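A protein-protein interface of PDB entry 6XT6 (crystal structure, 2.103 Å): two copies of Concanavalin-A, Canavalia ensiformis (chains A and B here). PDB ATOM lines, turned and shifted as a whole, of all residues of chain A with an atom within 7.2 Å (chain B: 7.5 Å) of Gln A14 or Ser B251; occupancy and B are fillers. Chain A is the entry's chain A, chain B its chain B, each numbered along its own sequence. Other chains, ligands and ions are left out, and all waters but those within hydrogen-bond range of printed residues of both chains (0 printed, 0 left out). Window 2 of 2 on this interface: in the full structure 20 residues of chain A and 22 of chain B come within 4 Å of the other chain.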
ATOM      1  N   MET A  11      20.323 -10.413  16.474  1.00  0.00           N
ATOM      2  CA  MET A  11      19.689 -11.390  15.563  1.00  0.00           C
ATOM      3  C   MET A  11      20.384 -11.327  14.198  1.00  0.00           C
ATOM      4  O   MET A  11      20.391 -10.254  13.566  1.00  0.00           O
ATOM      5  CB  MET A  11      18.205 -11.070  15.422  1.00  0.00           C
ATOM      6  CG  MET A  11      17.433 -12.140  14.680  1.00  0.00           C
ATOM      7  SD  MET A  11      15.662 -11.929  14.958  1.00  0.00           S
ATOM      8  CE  MET A  11      15.356 -10.325  14.217  1.00  0.00           C
ATOM      9  N   PHE A  12      20.991 -12.444  13.799  1.00  0.00           N
ATOM     10  CA  PHE A  12      21.458 -12.753  12.424  1.00  0.00           C
ATOM     11  C   PHE A  12      20.456 -13.711  11.778  1.00  0.00           C
ATOM     12  O   PHE A  12      20.335 -14.845  12.260  1.00  0.00           O
ATOM     13  CB  PHE A  12      22.853 -13.381  12.465  1.00  0.00           C
ATOM     14  CG  PHE A  12      23.911 -12.561  13.161  1.00  0.00           C
ATOM     15  CD1 PHE A  12      24.624 -11.588  12.479  1.00  0.00           C
ATOM     16  CD2 PHE A  12      24.225 -12.785  14.491  1.00  0.00           C
ATOM     17  CE1 PHE A  12      25.614 -10.859  13.113  1.00  0.00           C
ATOM     18  CE2 PHE A  12      25.219 -12.053  15.121  1.00  0.00           C
ATOM     19  CZ  PHE A  12      25.906 -11.086  14.432  1.00  0.00           C
ATOM     20  N   ASN A  13      19.740 -13.265  10.749  1.00  0.00           N
ATOM     21  CA  ASN A  13      18.958 -14.168   9.860  1.00  0.00           C
ATOM     22  C   ASN A  13      19.695 -14.319   8.530  1.00  0.00           C
ATOM     23  O   ASN A  13      19.287 -15.137   7.707  1.00  0.00           O
ATOM     24  CB  ASN A  13      17.513 -13.694   9.688  1.00  0.00           C
ATOM     25  CG  ASN A  13      16.677 -14.101  10.881  1.00  0.00           C
ATOM     26  OD1 ASN A  13      16.575 -15.285  11.187  1.00  0.00           O
ATOM     27  ND2 ASN A  13      16.087 -13.135  11.568  1.00  0.00           N
ATOM     28  N   GLN A  14      20.766 -13.570   8.348  1.00  0.00           N
ATOM     29  CA  GLN A  14      21.604 -13.630   7.134  1.00  0.00           C
ATOM     30  C   GLN A  14      23.018 -13.240   7.556  1.00  0.00           C
ATOM     31  O   GLN A  14      23.141 -12.413   8.445  1.00  0.00           O
ATOM     32  CB  GLN A  14      20.977 -12.708   6.092  1.00  0.00           C
ATOM     33  CG  GLN A  14      21.776 -12.588   4.812  1.00  0.00           C
ATOM     34  CD  GLN A  14      20.904 -12.989   3.656  1.00  0.00           C
ATOM     35  OE1 GLN A  14      20.379 -12.141   2.931  1.00  0.00           O
ATOM     36  NE2 GLN A  14      20.711 -14.294   3.522  1.00  0.00           N
ATOM     37  N   PHE A  15      24.042 -13.883   7.013  1.00  0.00           N
ATOM     38  CA  PHE A  15      25.457 -13.498   7.244  1.00  0.00           C
ATOM     39  C   PHE A  15      26.002 -12.986   5.915  1.00  0.00           C
ATOM     40  O   PHE A  15      25.549 -13.474   4.870  1.00  0.00           O
ATOM     41  CB  PHE A  15      26.264 -14.676   7.792  1.00  0.00           C
ATOM     42  CG  PHE A  15      25.720 -15.241   9.077  1.00  0.00           C
ATOM     43  CD1 PHE A  15      26.115 -14.722  10.302  1.00  0.00           C
ATOM     44  CD2 PHE A  15      24.779 -16.255   9.063  1.00  0.00           C
ATOM     45  CE1 PHE A  15      25.615 -15.232  11.489  1.00  0.00           C
ATOM     46  CE2 PHE A  15      24.258 -16.752  10.253  1.00  0.00           C
ATOM     47  CZ  PHE A  15      24.676 -16.238  11.464  1.00  0.00           C
ATOM     48  N   SER A  16      26.923 -12.028   5.960  1.00  0.00           N
ATOM     49  CA  SER A  16      27.657 -11.545   4.770  1.00  0.00           C
ATOM     50  C   SER A  16      29.162 -11.737   4.980  1.00  0.00           C
ATOM     51  O   SER A  16      29.597 -11.970   6.136  1.00  0.00           O
ATOM     52  CB  SER A  16      27.283 -10.121   4.455  1.00  0.00           C
ATOM     53  OG  SER A  16      27.211  -9.351   5.641  1.00  0.00           O
ATOM     54  N   GLN A  19      31.403  -9.649   8.103  1.00  0.00           N
ATOM     55  CA  GLN A  19      30.409  -9.399   9.172  1.00  0.00           C
ATOM     56  C   GLN A  19      31.165  -8.743  10.332  1.00  0.00           C
ATOM     57  O   GLN A  19      31.714  -9.496  11.141  1.00  0.00           O
ATOM     58  CB  GLN A  19      29.762 -10.738   9.541  1.00  0.00           C
ATOM     59  CG  GLN A  19      28.489 -10.619  10.366  1.00  0.00           C
ATOM     60  CD  GLN A  19      27.325 -10.051   9.595  1.00  0.00           C
ATOM     61  OE1 GLN A  19      27.025 -10.477   8.482  1.00  0.00           O
ATOM     62  NE2 GLN A  19      26.630  -9.110  10.214  1.00  0.00           N
ATOM     63  N   GLY A  31      28.913 -15.810   4.593  1.00  0.00           N
ATOM     64  CA  GLY A  31      28.468 -15.180   3.335  1.00  0.00           C
ATOM     65  C   GLY A  31      28.053 -16.183   2.276  1.00  0.00           C
ATOM     66  O   GLY A  31      27.110 -15.870   1.528  1.00  0.00           O
ATOM     67  N   ASP A  33      25.979 -18.379   0.545  1.00  0.00           N
ATOM     68  CA  ASP A  33      24.494 -18.536   0.588  1.00  0.00           C
ATOM     69  C   ASP A  33      23.904 -17.807   1.801  1.00  0.00           C
ATOM     70  O   ASP A  33      22.775 -18.149   2.243  1.00  0.00           O
ATOM     71  CB  ASP A  33      24.087 -20.011   0.564  1.00  0.00           C
ATOM     72  CG  ASP A  33      24.144 -20.598  -0.832  1.00  0.00           C
ATOM     73  OD1 ASP A  33      23.060 -20.739  -1.451  1.00  0.00           O
ATOM     74  OD2 ASP A  33      25.274 -20.898  -1.294  1.00  0.00           O
ATOM     75  N   GLY A  34      24.630 -16.822   2.314  1.00  0.00           N
ATOM     76  CA  GLY A  34      24.186 -15.978   3.432  1.00  0.00           C
ATOM     77  C   GLY A  34      24.281 -16.717   4.747  1.00  0.00           C
ATOM     78  O   GLY A  34      23.565 -16.337   5.671  1.00  0.00           O
ATOM     79  N   ASN A  35      25.149 -17.725   4.826  1.00  0.00           N
ATOM     80  CA  ASN A  35      25.242 -18.642   5.985  1.00  0.00           C
ATOM     81  C   ASN A  35      26.629 -18.497   6.613  1.00  0.00           C
ATOM     82  O   ASN A  35      27.506 -17.868   5.997  1.00  0.00           O
ATOM     83  CB  ASN A  35      24.956 -20.096   5.607  1.00  0.00           C
ATOM     84  CG  ASN A  35      23.537 -20.340   5.125  1.00  0.00           C
ATOM     85  OD1 ASN A  35      22.595 -19.663   5.524  1.00  0.00           O
ATOM     86  ND2 ASN A  35      23.363 -21.324   4.258  1.00  0.00           N
ATOM     87  N   LEU A  36      26.760 -19.006   7.837  1.00  0.00           N
ATOM     88  CA  LEU A  36      28.007 -19.056   8.637  1.00  0.00           C
ATOM     89  C   LEU A  36      28.490 -20.506   8.560  1.00  0.00           C
ATOM     90  O   LEU A  36      27.736 -21.396   8.992  1.00  0.00           O
ATOM     91  CB  LEU A  36      27.671 -18.587  10.065  1.00  0.00           C
ATOM     92  CG  LEU A  36      28.689 -18.913  11.157  1.00  0.00           C
ATOM     93  CD1 LEU A  36      30.059 -18.347  10.826  1.00  0.00           C
ATOM     94  CD2 LEU A  36      28.221 -18.393  12.508  1.00  0.00           C
ATOM     95  N   LEU A 241      22.337 -21.002   9.987  1.00  0.00           N
ATOM     96  CA  LEU A 241      21.459 -20.219   9.066  1.00  0.00           C
ATOM     97  C   LEU A 241      20.926 -18.986   9.790  1.00  0.00           C
ATOM     98  O   LEU A 241      20.592 -18.002   9.105  1.00  0.00           O
ATOM     99  CB  LEU A 241      20.309 -21.082   8.539  1.00  0.00           C
ATOM    100  CG  LEU A 241      20.703 -22.433   7.925  1.00  0.00           C
ATOM    101  CD1 LEU A 241      19.547 -23.019   7.146  1.00  0.00           C
ATOM    102  CD2 LEU A 241      21.903 -22.306   7.011  1.00  0.00           C
ATOM    103  N   SER A 242      20.884 -19.026  11.121  1.00  0.00           N
ATOM    104  CA  SER A 242      20.434 -17.899  11.965  1.00  0.00           C
ATOM    105  C   SER A 242      20.909 -18.094  13.406  1.00  0.00           C
ATOM    106  O   SER A 242      21.160 -19.237  13.810  1.00  0.00           O
ATOM    107  CB  SER A 242      18.948 -17.741  11.878  1.00  0.00           C
ATOM    108  OG  SER A 242      18.311 -18.838  12.500  1.00  0.00           O
ATOM    109  N   TRP A 243      21.043 -16.989  14.131  1.00  0.00           N
ATOM    110  CA  TRP A 243      21.558 -16.941  15.512  1.00  0.00           C
ATOM    111  C   TRP A 243      21.077 -15.655  16.163  1.00  0.00           C
ATOM    112  O   TRP A 243      21.405 -14.564  15.663  1.00  0.00           O
ATOM    113  CB  TRP A 243      23.080 -17.037  15.513  1.00  0.00           C
ATOM    114  CG  TRP A 243      23.707 -16.985  16.868  1.00  0.00           C
ATOM    115  CD1 TRP A 243      23.200 -17.450  18.047  1.00  0.00           C
ATOM    116  CD2 TRP A 243      25.011 -16.468  17.164  1.00  0.00           C
ATOM    117  NE1 TRP A 243      24.104 -17.250  19.058  1.00  0.00           N
ATOM    118  CE2 TRP A 243      25.222 -16.652  18.544  1.00  0.00           C
ATOM    119  CE3 TRP A 243      26.010 -15.856  16.399  1.00  0.00           C
ATOM    120  CZ2 TRP A 243      26.401 -16.245  19.169  1.00  0.00           C
ATOM    121  CZ3 TRP A 243      27.171 -15.458  17.016  1.00  0.00           C
ATOM    122  CH2 TRP A 243      27.358 -15.649  18.383  1.00  0.00           C
ATOM    123  N   HIS B   3      10.895 -13.298   9.625  1.00  0.00           N
ATOM    124  CA  HIS B   3      12.085 -14.033  10.135  1.00  0.00           C
ATOM    125  C   HIS B   3      13.342 -13.702   9.307  1.00  0.00           C
ATOM    126  O   HIS B   3      14.271 -14.540   9.298  1.00  0.00           O
ATOM    127  CB  HIS B   3      11.753 -15.525  10.002  1.00  0.00           C
ATOM    128  CG  HIS B   3      11.054 -15.785   8.709  1.00  0.00           C
ATOM    129  ND1 HIS B   3      11.678 -16.387   7.631  1.00  0.00           N
ATOM    130  CD2 HIS B   3       9.820 -15.423   8.280  1.00  0.00           C
ATOM    131  CE1 HIS B   3      10.843 -16.438   6.612  1.00  0.00           C
ATOM    132  NE2 HIS B   3       9.698 -15.841   6.983  1.00  0.00           N
ATOM    133  N   GLU B   4      13.357 -12.560   8.602  1.00  0.00           N
ATOM    134  CA  GLU B   4      14.295 -12.248   7.483  1.00  0.00           C
ATOM    135  C   GLU B   4      15.068 -10.957   7.804  1.00  0.00           C
ATOM    136  O   GLU B   4      15.553 -10.285   6.886  1.00  0.00           O
ATOM    137  CB  GLU B   4      13.499 -12.130   6.179  1.00  0.00           C
ATOM    138  CG  GLU B   4      12.726 -13.394   5.814  1.00  0.00           C
ATOM    139  CD  GLU B   4      11.462 -13.200   4.984  1.00  0.00           C
ATOM    140  OE1 GLU B   4      11.069 -14.161   4.304  1.00  0.00           O
ATOM    141  OE2 GLU B   4      10.852 -12.104   5.043  1.00  0.00           O
ATOM    142  N   THR B   5      15.225 -10.669   9.087  1.00  0.00           N
ATOM    143  CA  THR B   5      15.653  -9.368   9.640  1.00  0.00           C
ATOM    144  C   THR B   5      16.934  -9.578  10.457  1.00  0.00           C
ATOM    145  O   THR B   5      16.942 -10.494  11.297  1.00  0.00           O
ATOM    146  CB  THR B   5      14.493  -8.818  10.474  1.00  0.00           C
ATOM    147  OG1 THR B   5      13.449  -8.565   9.533  1.00  0.00           O
ATOM    148  CG2 THR B   5      14.817  -7.559  11.244  1.00  0.00           C
ATOM    149  N   ASN B   6      17.970  -8.777  10.209  1.00  0.00           N
ATOM    150  CA  ASN B   6      19.133  -8.617  11.121  1.00  0.00           C
ATOM    151  C   ASN B   6      18.802  -7.487  12.111  1.00  0.00           C
ATOM    152  O   ASN B   6      18.121  -6.527  11.687  1.00  0.00           O
ATOM    153  CB  ASN B   6      20.402  -8.415  10.305  1.00  0.00           C
ATOM    154  CG  ASN B   6      20.906  -9.714   9.708  1.00  0.00           C
ATOM    155  OD1 ASN B   6      20.164 -10.684   9.566  1.00  0.00           O
ATOM    156  ND2 ASN B   6      22.198  -9.768   9.434  1.00  0.00           N
ATOM    157  N   HIS B  62      25.384  -2.422  11.123  1.00  0.00           N
ATOM    158  CA  HIS B  62      25.225  -2.547   9.652  1.00  0.00           C
ATOM    159  C   HIS B  62      24.016  -1.706   9.209  1.00  0.00           C
ATOM    160  O   HIS B  62      22.881  -2.116   9.467  1.00  0.00           O
ATOM    161  CB  HIS B  62      25.056  -4.029   9.274  1.00  0.00           C
ATOM    162  CG  HIS B  62      25.337  -4.332   7.842  1.00  0.00           C
ATOM    163  ND1 HIS B  62      25.095  -5.565   7.298  1.00  0.00           N
ATOM    164  CD2 HIS B  62      25.856  -3.575   6.854  1.00  0.00           C
ATOM    165  CE1 HIS B  62      25.445  -5.562   6.030  1.00  0.00           C
ATOM    166  NE2 HIS B  62      25.922  -4.346   5.727  1.00  0.00           N
ATOM    167  N   GLU B  65      23.176  -1.783   2.672  1.00  0.00           N
ATOM    168  CA  GLU B  65      23.795  -2.856   1.859  1.00  0.00           C
ATOM    169  C   GLU B  65      23.771  -2.442   0.397  1.00  0.00           C
ATOM    170  O   GLU B  65      23.015  -1.536   0.057  1.00  0.00           O
ATOM    171  CB  GLU B  65      23.044  -4.163   2.074  1.00  0.00           C
ATOM    172  CG  GLU B  65      23.379  -4.789   3.404  1.00  0.00           C
ATOM    173  CD  GLU B  65      22.623  -6.073   3.691  1.00  0.00           C
ATOM    174  OE1 GLU B  65      21.464  -6.202   3.207  1.00  0.00           O
ATOM    175  OE2 GLU B  65      23.190  -6.941   4.402  1.00  0.00           O
ATOM    176  N   SER B  67      22.496  -3.354  -2.163  1.00  0.00           N
ATOM    177  CA  SER B  67      21.093  -3.398  -2.663  1.00  0.00           C
ATOM    178  C   SER B  67      20.325  -2.082  -2.463  1.00  0.00           C
ATOM    179  O   SER B  67      19.154  -2.014  -2.925  1.00  0.00           O
ATOM    180  CB  SER B  67      20.379  -4.491  -1.934  1.00  0.00           C
ATOM    181  OG  SER B  67      20.523  -4.303  -0.531  1.00  0.00           O
ATOM    182  N   VAL B  69      19.219  -1.242   0.330  1.00  0.00           N
ATOM    183  CA  VAL B  69      18.410  -1.525   1.545  1.00  0.00           C
ATOM    184  C   VAL B  69      19.106  -0.815   2.706  1.00  0.00           C
ATOM    185  O   VAL B  69      20.344  -1.039   2.901  1.00  0.00           O
ATOM    186  CB  VAL B  69      18.267  -3.031   1.836  1.00  0.00           C
ATOM    187  CG1 VAL B  69      17.493  -3.250   3.127  1.00  0.00           C
ATOM    188  CG2 VAL B  69      17.615  -3.786   0.683  1.00  0.00           C
ATOM    189  N   LYS B 248      17.252  -2.307  12.821  1.00  0.00           N
ATOM    190  CA  LYS B 248      16.723  -3.442  12.017  1.00  0.00           C
ATOM    191  C   LYS B 248      17.039  -3.251  10.527  1.00  0.00           C
ATOM    192  O   LYS B 248      16.722  -2.195   9.980  1.00  0.00           O
ATOM    193  CB  LYS B 248      15.228  -3.602  12.305  1.00  0.00           C
ATOM    194  CG  LYS B 248      14.945  -4.275  13.644  1.00  0.00           C
ATOM    195  CD  LYS B 248      13.592  -4.001  14.238  1.00  0.00           C
ATOM    196  CE  LYS B 248      13.281  -4.924  15.398  1.00  0.00           C
ATOM    197  NZ  LYS B 248      11.816  -5.059  15.587  1.00  0.00           N
ATOM    198  N   LEU B 249      17.608  -4.280   9.901  1.00  0.00           N
ATOM    199  CA  LEU B 249      17.957  -4.341   8.457  1.00  0.00           C
ATOM    200  C   LEU B 249      17.310  -5.595   7.832  1.00  0.00           C
ATOM    201  O   LEU B 249      17.696  -6.723   8.212  1.00  0.00           O
ATOM    202  CB  LEU B 249      19.487  -4.383   8.408  1.00  0.00           C
ATOM    203  CG  LEU B 249      20.141  -4.414   7.036  1.00  0.00           C
ATOM    204  CD1 LEU B 249      19.770  -3.195   6.243  1.00  0.00           C
ATOM    205  CD2 LEU B 249      21.653  -4.510   7.179  1.00  0.00           C
ATOM    206  N   LYS B 250      16.322  -5.443   6.948  1.00  0.00           N
ATOM    207  CA  LYS B 250      15.704  -6.608   6.251  1.00  0.00           C
ATOM    208  C   LYS B 250      16.249  -6.666   4.832  1.00  0.00           C
ATOM    209  O   LYS B 250      15.786  -5.878   3.990  1.00  0.00           O
ATOM    210  CB  LYS B 250      14.182  -6.504   6.268  1.00  0.00           C
ATOM    211  CG  LYS B 250      13.404  -7.714   5.746  1.00  0.00           C
ATOM    212  CD  LYS B 250      11.892  -7.569   5.968  1.00  0.00           C
ATOM    213  CE  LYS B 250      11.049  -8.714   5.432  1.00  0.00           C
ATOM    214  NZ  LYS B 250      11.125  -8.824   3.955  1.00  0.00           N
ATOM    215  N   SER B 251      17.229  -7.542   4.611  1.00  0.00           N
ATOM    216  CA  SER B 251      18.089  -7.603   3.400  1.00  0.00           C
ATOM    217  C   SER B 251      17.281  -7.992   2.154  1.00  0.00           C
ATOM    218  O   SER B 251      17.668  -7.568   1.043  1.00  0.00           O
ATOM    219  CB  SER B 251      19.235  -8.544   3.629  1.00  0.00           C
ATOM    220  OG  SER B 251      19.975  -8.163   4.791  1.00  0.00           O
ATOM    221  N   ASN B 252      16.206  -8.769   2.304  1.00  0.00           N
ATOM    222  CA  ASN B 252      15.361  -9.182   1.153  1.00  0.00           C
ATOM    223  C   ASN B 252      14.156  -8.235   1.022  1.00  0.00           C
ATOM    224  O   ASN B 252      13.232  -8.575   0.266  1.00  0.00           O
ATOM    225  CB  ASN B 252      14.937 -10.651   1.258  1.00  0.00           C
ATOM    226  CG  ASN B 252      13.842 -10.883   2.280  1.00  0.00           C
ATOM    227  OD1 ASN B 252      13.387  -9.950   2.938  1.00  0.00           O
ATOM    228  ND2 ASN B 252      13.423 -12.130   2.435  1.00  0.00           N
ATOM    229  N   GLU B 253      14.147  -7.090   1.716  1.00  0.00           N
ATOM    230  CA  GLU B 253      13.032  -6.099   1.646  1.00  0.00           C
ATOM    231  C   GLU B 253      13.182  -5.268   0.364  1.00  0.00           C
ATOM    232  O   GLU B 253      14.325  -5.077  -0.111  1.00  0.00           O
ATOM    233  CB  GLU B 253      12.999  -5.219   2.904  1.00  0.00           C
ATOM    234  CG  GLU B 253      11.760  -4.332   3.034  1.00  0.00           C
ATOM    235  CD  GLU B 253      10.423  -5.034   3.255  1.00  0.00           C
ATOM    236  OE1 GLU B 253      10.399  -6.281   3.405  1.00  0.00           O
ATOM    237  OE2 GLU B 253       9.390  -4.331   3.285  1.00  0.00           O
ATOM    238  N   ILE B 254      12.070  -4.787  -0.194  1.00  0.00           N
ATOM    239  CA  ILE B 254      12.121  -3.764  -1.276  1.00  0.00           C
ATOM    240  C   ILE B 254      12.894  -2.570  -0.701  1.00  0.00           C
ATOM    241  O   ILE B 254      12.622  -2.132   0.411  1.00  0.00           O
ATOM    242  CB  ILE B 254      10.703  -3.413  -1.798  1.00  0.00           C
ATOM    243  CG1 ILE B 254      10.775  -2.783  -3.196  1.00  0.00           C
ATOM    244  CG2 ILE B 254       9.961  -2.531  -0.803  1.00  0.00           C
ATOM    245  CD1 ILE B 254       9.440  -2.484  -3.835  1.00  0.00           C
ATOM    246  N   PRO B 255      13.939  -2.046  -1.383  1.00  0.00           N
ATOM    247  CA  PRO B 255      14.770  -0.995  -0.793  1.00  0.00           C
ATOM    248  C   PRO B 255      14.098   0.386  -0.727  1.00  0.00           C
ATOM    249  O   PRO B 255      14.548   1.185   0.032  1.00  0.00           O
ATOM    250  CB  PRO B 255      16.024  -0.970  -1.690  1.00  0.00           C
ATOM    251  CG  PRO B 255      15.529  -1.491  -3.037  1.00  0.00           C
ATOM    252  CD  PRO B 255      14.413  -2.470  -2.711  1.00  0.00           C
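The side-chain amide oxygen of Asn A13 lies close to the backbone carbonyl oxygen of His B3, at 3.1 Å. ND2 of Asn A13 is in hydrogen-bond range of O of Thr B5 (2.8 Å). OD1 of Asn B6 is in hydrogen-bond range of N of Asn A13, at 2.9 Å. The side-chain amide nitrogen of Asn B6 is in hydrogen-bond range of the backbone carbonyl oxygen of Gln A14, at 3.0 Å.
Of the 15 printed residues of chain A, 4 touch a printed residue of chain B. Hydrophobic or aromatic side chains of chain A that line the printed part of chain B: Met A11. Among the printed residues, 8 pairs touch across the chains. Among the printed residues, no Asp or Glu carboxylate lies within 4 Å of a Lys or Arg side-chain nitrogen of the other chain.
Among the printed residues, pairs that only touch across the chains: Met A11 with Asn B6 (3.2 Å), Met A11 with Thr B5 (3.3 Å), Phe A12 with Asn B6 (3.8 Å) and Gln A14 with Ser B251 (3.8 Å).
The side-chain sulfur (SD) of Met A11 sits close to the side-chain amide nitrogen (ND2) of Asn A13, 3.6 Å away. The backbone carbonyl oxygen (O) of Trp A243 sits at hydrogen-bond distance from the backbone NH (N) of Phe A12 (2.9 Å). A ring nitrogen (NE2) of His B3 lies close to the side-chain carboxylate (OE1) of Glu B4 (3.4 Å). N of Asn B6 sits at hydrogen-bond distance from O of Leu B249 (2.9 Å). The side-chain hydroxyl of Ser B251 is in hydrogen-bond range of the side-chain carboxylate of Glu B65, at 2.9 Å.
Of the printed residues of chain B, Met A11 touches Thr B5 and Asn B6. Of the printed residues of chain B, Phe A12 touches Asn B6. Gln A14 touches just these residues of chain B: Asn B6 and Ser B251. Asn A35 touches none of the printed residues of chain B. Leu A36 touches none of the printed residues of chain B. Of the printed residues of chain A, His B3 touches Asn A13 (2.9 Å). Printed residues of chain A within 4 Å of Thr B5: Met A11 (3.3 Å) and Asn A13 (2.8 Å). Of the printed residues of chain A, Asn B6 touches Met A11, Phe A12, Asn A13 and Gln A14. Of chain A, only Gln A14 comes within 4 Å of Ser B251. The nearest residue of chain B that does not touch Gln A14 is Asn B252 (5.4 Å). The nearest printed residue of chain A that does not touch Ser B251 is Asn A13 (7.2 Å).
No position is printed for both chains. Of the 8 pairs that touch across the chains among the printed residues, none has its exchanged pair printed and touching as well.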
